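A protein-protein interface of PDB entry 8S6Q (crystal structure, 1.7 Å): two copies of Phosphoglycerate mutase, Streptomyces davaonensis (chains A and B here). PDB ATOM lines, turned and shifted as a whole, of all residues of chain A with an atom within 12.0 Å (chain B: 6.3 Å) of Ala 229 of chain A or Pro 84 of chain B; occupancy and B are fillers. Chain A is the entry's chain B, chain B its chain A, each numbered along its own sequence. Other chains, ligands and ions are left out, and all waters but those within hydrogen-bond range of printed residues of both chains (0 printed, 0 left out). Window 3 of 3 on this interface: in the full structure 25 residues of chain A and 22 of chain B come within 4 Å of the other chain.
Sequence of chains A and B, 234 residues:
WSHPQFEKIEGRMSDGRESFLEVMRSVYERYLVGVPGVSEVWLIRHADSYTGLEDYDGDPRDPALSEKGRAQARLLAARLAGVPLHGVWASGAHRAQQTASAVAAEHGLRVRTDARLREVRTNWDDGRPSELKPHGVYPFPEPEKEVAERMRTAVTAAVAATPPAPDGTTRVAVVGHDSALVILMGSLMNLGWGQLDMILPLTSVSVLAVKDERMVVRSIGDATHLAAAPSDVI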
ATOM      1  N   ALA A  71     -22.633  -6.552   0.940  1.00  0.00           N
ATOM      2  CA  ALA A  71     -22.838  -7.571  -0.096  1.00  0.00           C
ATOM      3  C   ALA A  71     -22.976  -8.973   0.495  1.00  0.00           C
ATOM      4  O   ALA A  71     -23.793  -9.774   0.019  1.00  0.00           O
ATOM      5  CB  ALA A  71     -21.692  -7.551  -1.122  1.00  0.00           C
ATOM      6  N   GLN A  72     -22.133  -9.317   1.473  1.00  0.00           N
ATOM      7  CA  GLN A  72     -22.259 -10.637   2.100  1.00  0.00           C
ATOM      8  C   GLN A  72     -23.594 -10.734   2.822  1.00  0.00           C
ATOM      9  O   GLN A  72     -24.295 -11.745   2.725  1.00  0.00           O
ATOM     10  CB  GLN A  72     -21.111 -10.894   3.095  1.00  0.00           C
ATOM     11  CG  GLN A  72     -19.701 -10.848   2.505  1.00  0.00           C
ATOM     12  CD  GLN A  72     -18.674 -10.819   3.621  1.00  0.00           C
ATOM     13  OE1 GLN A  72     -18.981 -10.372   4.719  1.00  0.00           O
ATOM     14  NE2 GLN A  72     -17.450 -11.245   3.337  1.00  0.00           N
ATOM     15  N   ARG A  74     -26.327  -9.244   2.072  1.00  0.00           N
ATOM     16  CA  ARG A  74     -27.416  -9.373   1.107  1.00  0.00           C
ATOM     17  C   ARG A  74     -27.561 -10.821   0.680  1.00  0.00           C
ATOM     18  O   ARG A  74     -28.682 -11.343   0.568  1.00  0.00           O
ATOM     19  CB  ARG A  74     -27.173  -8.463  -0.124  1.00  0.00           C
ATOM     20  CG  ARG A  74     -27.598  -7.013   0.170  1.00  0.00           C
ATOM     21  CD  ARG A  74     -27.680  -6.117  -1.076  1.00  0.00           C
ATOM     22  NE  ARG A  74     -26.383  -6.014  -1.742  1.00  0.00           N
ATOM     23  CZ  ARG A  74     -25.464  -5.103  -1.444  1.00  0.00           C
ATOM     24  NH1 ARG A  74     -25.720  -4.121  -0.603  1.00  0.00           N
ATOM     25  NH2 ARG A  74     -24.266  -5.173  -2.019  1.00  0.00           N
ATOM     26  N   LEU A  75     -26.422 -11.499   0.470  1.00  0.00           N
ATOM     27  CA  LEU A  75     -26.456 -12.885   0.036  1.00  0.00           C
ATOM     28  C   LEU A  75     -27.030 -13.766   1.128  1.00  0.00           C
ATOM     29  O   LEU A  75     -27.840 -14.662   0.843  1.00  0.00           O
ATOM     30  CB  LEU A  75     -25.056 -13.341  -0.366  1.00  0.00           C
ATOM     31  CG  LEU A  75     -24.514 -12.610  -1.595  1.00  0.00           C
ATOM     32  CD1 LEU A  75     -22.999 -12.724  -1.763  1.00  0.00           C
ATOM     33  CD2 LEU A  75     -25.227 -13.154  -2.791  1.00  0.00           C
ATOM     34  N   LEU A  76     -26.600 -13.521   2.391  1.00  0.00           N
ATOM     35  CA  LEU A  76     -27.137 -14.245   3.533  1.00  0.00           C
ATOM     36  C   LEU A  76     -28.636 -14.016   3.666  1.00  0.00           C
ATOM     37  O   LEU A  76     -29.404 -14.967   3.840  1.00  0.00           O
ATOM     38  CB  LEU A  76     -26.400 -13.812   4.822  1.00  0.00           C
ATOM     39  CG  LEU A  76     -26.943 -14.369   6.132  1.00  0.00           C
ATOM     40  CD1 LEU A  76     -26.494 -15.845   6.224  1.00  0.00           C
ATOM     41  CD2 LEU A  76     -26.462 -13.510   7.327  1.00  0.00           C
ATOM     42  N   ALA A  78     -30.727 -13.213   1.315  1.00  0.00           N
ATOM     43  CA  ALA A  78     -31.427 -13.918   0.260  1.00  0.00           C
ATOM     44  C   ALA A  78     -31.448 -15.415   0.544  1.00  0.00           C
ATOM     45  O   ALA A  78     -32.433 -16.096   0.224  1.00  0.00           O
ATOM     46  CB  ALA A  78     -30.797 -13.608  -1.096  1.00  0.00           C
ATOM     47  N   ARG A  79     -30.366 -15.956   1.112  1.00  0.00           N
ATOM     48  CA  ARG A  79     -30.379 -17.385   1.436  1.00  0.00           C
ATOM     49  C   ARG A  79     -31.435 -17.702   2.491  1.00  0.00           C
ATOM     50  O   ARG A  79     -32.166 -18.688   2.378  1.00  0.00           O
ATOM     51  CB  ARG A  79     -28.997 -17.829   1.909  1.00  0.00           C
ATOM     52  CG  ARG A  79     -29.000 -19.164   2.613  1.00  0.00           C
ATOM     53  CD  ARG A  79     -27.645 -19.336   3.318  1.00  0.00           C
ATOM     54  NE  ARG A  79     -27.515 -20.707   3.814  1.00  0.00           N
ATOM     55  CZ  ARG A  79     -26.409 -21.258   4.305  1.00  0.00           C
ATOM     56  NH1 ARG A  79     -25.252 -20.622   4.310  1.00  0.00           N
ATOM     57  NH2 ARG A  79     -26.452 -22.516   4.722  1.00  0.00           N
ATOM     58  N   ALA A 223     -20.749 -21.029   4.749  1.00  0.00           N
ATOM     59  CA  ALA A 223     -20.876 -19.747   4.074  1.00  0.00           C
ATOM     60  C   ALA A 223     -21.057 -19.960   2.580  1.00  0.00           C
ATOM     61  O   ALA A 223     -20.608 -19.151   1.798  1.00  0.00           O
ATOM     62  CB  ALA A 223     -19.649 -18.885   4.352  1.00  0.00           C
ATOM     63  N   THR A 224     -21.657 -21.081   2.180  1.00  0.00           N
ATOM     64  CA  THR A 224     -21.747 -21.430   0.767  1.00  0.00           C
ATOM     65  C   THR A 224     -22.532 -20.403  -0.045  1.00  0.00           C
ATOM     66  O   THR A 224     -22.409 -20.406  -1.270  1.00  0.00           O
ATOM     67  CB  THR A 224     -22.371 -22.814   0.596  1.00  0.00           C
ATOM     68  OG1 THR A 224     -23.633 -22.846   1.261  1.00  0.00           O
ATOM     69  CG2 THR A 224     -21.450 -23.910   1.197  1.00  0.00           C
ATOM     70  N   HIS A 225     -23.300 -19.515   0.592  1.00  0.00           N
ATOM     71  CA  HIS A 225     -24.018 -18.483  -0.171  1.00  0.00           C
ATOM     72  C   HIS A 225     -23.078 -17.428  -0.739  1.00  0.00           C
ATOM     73  O   HIS A 225     -23.466 -16.686  -1.640  1.00  0.00           O
ATOM     74  CB  HIS A 225     -25.068 -17.866   0.739  1.00  0.00           C
ATOM     75  CG  HIS A 225     -24.460 -17.326   2.012  1.00  0.00           C
ATOM     76  ND1 HIS A 225     -24.408 -18.074   3.171  1.00  0.00           N
ATOM     77  CD2 HIS A 225     -23.890 -16.131   2.301  1.00  0.00           C
ATOM     78  CE1 HIS A 225     -23.810 -17.369   4.117  1.00  0.00           C
ATOM     79  NE2 HIS A 225     -23.506 -16.176   3.629  1.00  0.00           N
ATOM     80  N   LEU A 226     -21.847 -17.349  -0.252  1.00  0.00           N
ATOM     81  CA  LEU A 226     -20.851 -16.468  -0.845  1.00  0.00           C
ATOM     82  C   LEU A 226     -20.225 -17.042  -2.107  1.00  0.00           C
ATOM     83  O   LEU A 226     -19.523 -16.305  -2.807  1.00  0.00           O
ATOM     84  CB  LEU A 226     -19.743 -16.172   0.157  1.00  0.00           C
ATOM     85  CG  LEU A 226     -20.219 -15.546   1.464  1.00  0.00           C
ATOM     86  CD1 LEU A 226     -19.023 -15.405   2.411  1.00  0.00           C
ATOM     87  CD2 LEU A 226     -20.910 -14.194   1.218  1.00  0.00           C
ATOM     88  N   ALA A 227     -20.465 -18.319  -2.432  1.00  0.00           N
ATOM     89  CA  ALA A 227     -20.047 -18.832  -3.730  1.00  0.00           C
ATOM     90  C   ALA A 227     -21.030 -18.503  -4.846  1.00  0.00           C
ATOM     91  O   ALA A 227     -20.667 -18.635  -6.024  1.00  0.00           O
ATOM     92  CB  ALA A 227     -19.873 -20.342  -3.679  1.00  0.00           C
ATOM     93  N   ALA A 228     -22.266 -18.123  -4.506  1.00  0.00           N
ATOM     94  CA  ALA A 228     -23.328 -17.993  -5.500  1.00  0.00           C
ATOM     95  C   ALA A 228     -22.995 -16.882  -6.481  1.00  0.00           C
ATOM     96  O   ALA A 228     -22.896 -15.712  -6.095  1.00  0.00           O
ATOM     97  CB  ALA A 228     -24.671 -17.723  -4.819  1.00  0.00           C
ATOM     98  N   ALA A 229     -22.792 -17.262  -7.743  1.00  0.00           N
ATOM     99  CA  ALA A 229     -22.553 -16.320  -8.838  1.00  0.00           C
ATOM    100  C   ALA A 229     -23.867 -15.769  -9.382  1.00  0.00           C
ATOM    101  O   ALA A 229     -24.762 -16.532  -9.749  1.00  0.00           O
ATOM    102  CB  ALA A 229     -21.758 -16.995  -9.960  1.00  0.00           C
ATOM    103  N   LEU B  80     -27.427 -26.337  -5.198  1.00  0.00           N
ATOM    104  CA  LEU B  80     -26.112 -26.337  -5.826  1.00  0.00           C
ATOM    105  C   LEU B  80     -26.177 -25.811  -7.253  1.00  0.00           C
ATOM    106  O   LEU B  80     -25.120 -25.538  -7.835  1.00  0.00           O
ATOM    107  CB  LEU B  80     -25.493 -27.733  -5.824  1.00  0.00           C
ATOM    108  CG  LEU B  80     -24.549 -28.037  -4.623  1.00  0.00           C
ATOM    109  CD1 LEU B  80     -25.137 -27.593  -3.307  1.00  0.00           C
ATOM    110  CD2 LEU B  80     -24.207 -29.511  -4.565  1.00  0.00           C
ATOM    111  N   ALA B  81     -27.373 -25.720  -7.803  1.00  0.00           N
ATOM    112  CA  ALA B  81     -27.539 -25.153  -9.142  1.00  0.00           C
ATOM    113  C   ALA B  81     -26.992 -23.741  -9.222  1.00  0.00           C
ATOM    114  O   ALA B  81     -26.606 -23.297 -10.317  1.00  0.00           O
ATOM    115  CB  ALA B  81     -29.011 -25.150  -9.545  1.00  0.00           C
ATOM    116  N   GLY B  82     -26.967 -23.023  -8.091  1.00  0.00           N
ATOM    117  CA  GLY B  82     -26.656 -21.611  -8.041  1.00  0.00           C
ATOM    118  C   GLY B  82     -25.210 -21.341  -7.788  1.00  0.00           C
ATOM    119  O   GLY B  82     -24.792 -20.188  -7.694  1.00  0.00           O
ATOM    120  N   VAL B  83     -24.433 -22.413  -7.657  1.00  0.00           N
ATOM    121  CA  VAL B  83     -23.010 -22.355  -7.427  1.00  0.00           C
ATOM    122  C   VAL B  83     -22.219 -22.809  -8.638  1.00  0.00           C
ATOM    123  O   VAL B  83     -22.551 -23.841  -9.224  1.00  0.00           O
ATOM    124  CB  VAL B  83     -22.667 -23.262  -6.229  1.00  0.00           C
ATOM    125  CG1 VAL B  83     -21.237 -23.123  -5.865  1.00  0.00           C
ATOM    126  CG2 VAL B  83     -23.562 -22.843  -5.060  1.00  0.00           C
ATOM    127  N   PRO B  84     -21.090 -22.190  -8.937  1.00  0.00           N
ATOM    128  CA  PRO B  84     -20.202 -22.743  -9.975  1.00  0.00           C
ATOM    129  C   PRO B  84     -19.626 -24.077  -9.541  1.00  0.00           C
ATOM    130  O   PRO B  84     -19.197 -24.232  -8.401  1.00  0.00           O
ATOM    131  CB  PRO B  84     -19.100 -21.691 -10.100  1.00  0.00           C
ATOM    132  CG  PRO B  84     -19.759 -20.389  -9.579  1.00  0.00           C
ATOM    133  CD  PRO B  84     -20.668 -20.856  -8.467  1.00  0.00           C
ATOM    134  N   LEU B  85     -19.627 -25.043 -10.451  1.00  0.00           N
ATOM    135  CA  LEU B  85     -19.182 -26.395 -10.122  1.00  0.00           C
ATOM    136  C   LEU B  85     -18.442 -26.991 -11.304  1.00  0.00           C
ATOM    137  O   LEU B  85     -18.901 -26.886 -12.443  1.00  0.00           O
ATOM    138  CB  LEU B  85     -20.357 -27.261  -9.779  1.00  0.00           C
ATOM    139  CG  LEU B  85     -20.231 -28.453  -8.915  1.00  0.00           C
ATOM    140  CD1 LEU B  85     -19.431 -28.185  -7.547  1.00  0.00           C
ATOM    141  CD2 LEU B  85     -21.626 -28.948  -8.656  1.00  0.00           C
ATOM    142  N   HIS B  86     -17.320 -27.681 -11.016  1.00  0.00           N
ATOM    143  CA  HIS B  86     -16.434 -28.078 -12.083  1.00  0.00           C
ATOM    144  C   HIS B  86     -16.212 -29.590 -12.176  1.00  0.00           C
ATOM    145  O   HIS B  86     -15.636 -30.057 -13.163  1.00  0.00           O
ATOM    146  CB  HIS B  86     -15.132 -27.268 -11.942  1.00  0.00           C
ATOM    147  CG  HIS B  86     -15.388 -25.787 -11.799  1.00  0.00           C
ATOM    148  ND1 HIS B  86     -15.529 -25.147 -10.580  1.00  0.00           N
ATOM    149  CD2 HIS B  86     -15.686 -24.846 -12.748  1.00  0.00           C
ATOM    150  CE1 HIS B  86     -15.823 -23.871 -10.777  1.00  0.00           C
ATOM    151  NE2 HIS B  86     -15.917 -23.661 -12.088  1.00  0.00           N
ATOM    152  N   HIS B 107     -25.394 -28.812 -14.068  1.00  0.00           N
ATOM    153  CA  HIS B 107     -24.147 -28.204 -14.441  1.00  0.00           C
ATOM    154  C   HIS B 107     -23.529 -28.730 -15.735  1.00  0.00           C
ATOM    155  O   HIS B 107     -22.469 -28.239 -16.125  1.00  0.00           O
ATOM    156  CB  HIS B 107     -23.126 -28.388 -13.276  1.00  0.00           C
ATOM    157  CG  HIS B 107     -23.507 -27.634 -12.046  1.00  0.00           C
ATOM    158  ND1 HIS B 107     -24.279 -28.165 -11.032  1.00  0.00           N
ATOM    159  CD2 HIS B 107     -23.293 -26.342 -11.719  1.00  0.00           C
ATOM    160  CE1 HIS B 107     -24.436 -27.256 -10.084  1.00  0.00           C
ATOM    161  NE2 HIS B 107     -23.863 -26.133 -10.487  1.00  0.00           N
ATOM    162  N   ASP B 167     -12.894 -18.865 -13.987  1.00  0.00           N
ATOM    163  CA  ASP B 167     -12.763 -17.711 -13.116  1.00  0.00           C
ATOM    164  C   ASP B 167     -13.060 -18.156 -11.699  1.00  0.00           C
ATOM    165  O   ASP B 167     -13.988 -18.942 -11.472  1.00  0.00           O
ATOM    166  CB  ASP B 167     -13.684 -16.562 -13.545  1.00  0.00           C
ATOM    167  CG  ASP B 167     -12.963 -15.226 -13.561  1.00  0.00           C
ATOM    168  OD1 ASP B 167     -11.708 -15.228 -13.574  1.00  0.00           O
ATOM    169  OD2 ASP B 167     -13.641 -14.175 -13.589  1.00  0.00           O
ATOM    170  N   THR B 169     -12.807 -19.894  -7.946  1.00  0.00           N
ATOM    171  CA  THR B 169     -12.411 -21.109  -7.259  1.00  0.00           C
ATOM    172  C   THR B 169     -12.886 -22.351  -8.016  1.00  0.00           C
ATOM    173  O   THR B 169     -14.075 -22.477  -8.321  1.00  0.00           O
ATOM    174  CB  THR B 169     -12.991 -21.089  -5.836  1.00  0.00           C
ATOM    175  OG1 THR B 169     -12.640 -19.845  -5.191  1.00  0.00           O
ATOM    176  CG2 THR B 169     -12.484 -22.246  -5.033  1.00  0.00           C
ATOM    177  N   THR B 170     -11.954 -23.263  -8.331  1.00  0.00           N
ATOM    178  CA  THR B 170     -12.355 -24.596  -8.771  1.00  0.00           C
ATOM    179  C   THR B 170     -13.086 -25.318  -7.668  1.00  0.00           C
ATOM    180  O   THR B 170     -12.582 -25.436  -6.540  1.00  0.00           O
ATOM    181  CB  THR B 170     -11.150 -25.403  -9.260  1.00  0.00           C
ATOM    182  OG1 THR B 170     -10.394 -24.608 -10.195  1.00  0.00           O
ATOM    183  CG2 THR B 170     -11.529 -26.772  -9.799  1.00  0.00           C
ATOM    184  N   ARG B 171     -14.284 -25.809  -7.993  1.00  0.00           N
ATOM    185  CA  ARG B 171     -15.138 -26.446  -6.993  1.00  0.00           C
ATOM    186  C   ARG B 171     -15.579 -27.825  -7.445  1.00  0.00           C
ATOM    187  O   ARG B 171     -16.078 -27.993  -8.571  1.00  0.00           O
ATOM    188  CB  ARG B 171     -16.351 -25.538  -6.721  1.00  0.00           C
ATOM    189  CG  ARG B 171     -17.277 -26.042  -5.614  1.00  0.00           C
ATOM    190  CD  ARG B 171     -18.308 -24.919  -5.383  1.00  0.00           C
ATOM    191  NE  ARG B 171     -17.698 -23.733  -4.785  1.00  0.00           N
ATOM    192  CZ  ARG B 171     -17.448 -22.577  -5.376  1.00  0.00           C
ATOM    193  NH1 ARG B 171     -17.845 -22.316  -6.625  1.00  0.00           N
ATOM    194  NH2 ARG B 171     -16.764 -21.655  -4.707  1.00  0.00           N
ATOM    195  N   VAL B 172     -15.427 -28.807  -6.546  1.00  0.00           N
ATOM    196  CA  VAL B 172     -15.723 -30.194  -6.874  1.00  0.00           C
ATOM    197  C   VAL B 172     -16.664 -30.756  -5.829  1.00  0.00           C
ATOM    198  O   VAL B 172     -16.376 -30.699  -4.617  1.00  0.00           O
ATOM    199  CB  VAL B 172     -14.447 -31.051  -6.969  1.00  0.00           C
ATOM    200  CG1 VAL B 172     -14.799 -32.463  -7.227  1.00  0.00           C
ATOM    201  CG2 VAL B 172     -13.557 -30.468  -8.083  1.00  0.00           C
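No position is printed for both chains. Of the 6 pairs that touch across the chains among the printed residues, none has its exchanged pair printed and touching as well.
Ala 229 of chain A touches just these residues of chain B: Gly 82 and Pro 84. Of the printed residues of chain A, Pro 84 of chain B touches Ala 227 and Ala 229. Gly 82 of chain B touches just these residues of chain A: Ala 228 and Ala 229. Of chain A, only Ala 227 comes within 4 Å of Val 83 of chain B. No residue of chain A comes within 4 Å of Leu 85 of chain B. Of the printed residues of chain B, Ala 227 of chain A touches Val 83 (3.8 Å), Pro 84 (3.3 Å) and Arg 171 (3.5 Å). Of the printed residues of chain B, Ala 228 of chain A touches Gly 82. The nearest printed residue of chain B that does not touch Ala 228 of chain A is Val 83 of chain B (4.8 Å).
Among the printed residues, merely in contact across the chains: Ala 227 of chain A with Val 83 of chain B (3.8 Å), Ala 227 of chain A with Pro 84 of chain B (3.3 Å), Ala 227 of chain A with Arg 171 of chain B (3.5 Å), Ala 228 of chain A with Gly 82 of chain B (3.4 Å), Ala 229 of chain A with Gly 82 of chain B (3.5 Å) and Ala 229 of chain A with Pro 84 of chain B (3.96 Å).
Hydrophobic or aromatic side chains of chain A that line the printed part of chain B: Ala 227, Ala 228 and Ala 229. Hydrophobic or aromatic side chains of chain B that line the printed part of chain A: Val 83 and Pro 84.
The backbone carbonyl oxygen (O) of Val 83 of chain B sits at hydrogen-bond distance from a ring nitrogen (NE2) of His 107 of chain B. O of Pro 84 of chain B sits at hydrogen-bond distance from NH1 of Arg 171 of chain B (2.9 Å). O of Arg 171 of chain B lies within hydrogen-bond range of N of His 86 of chain B (2.8 Å).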
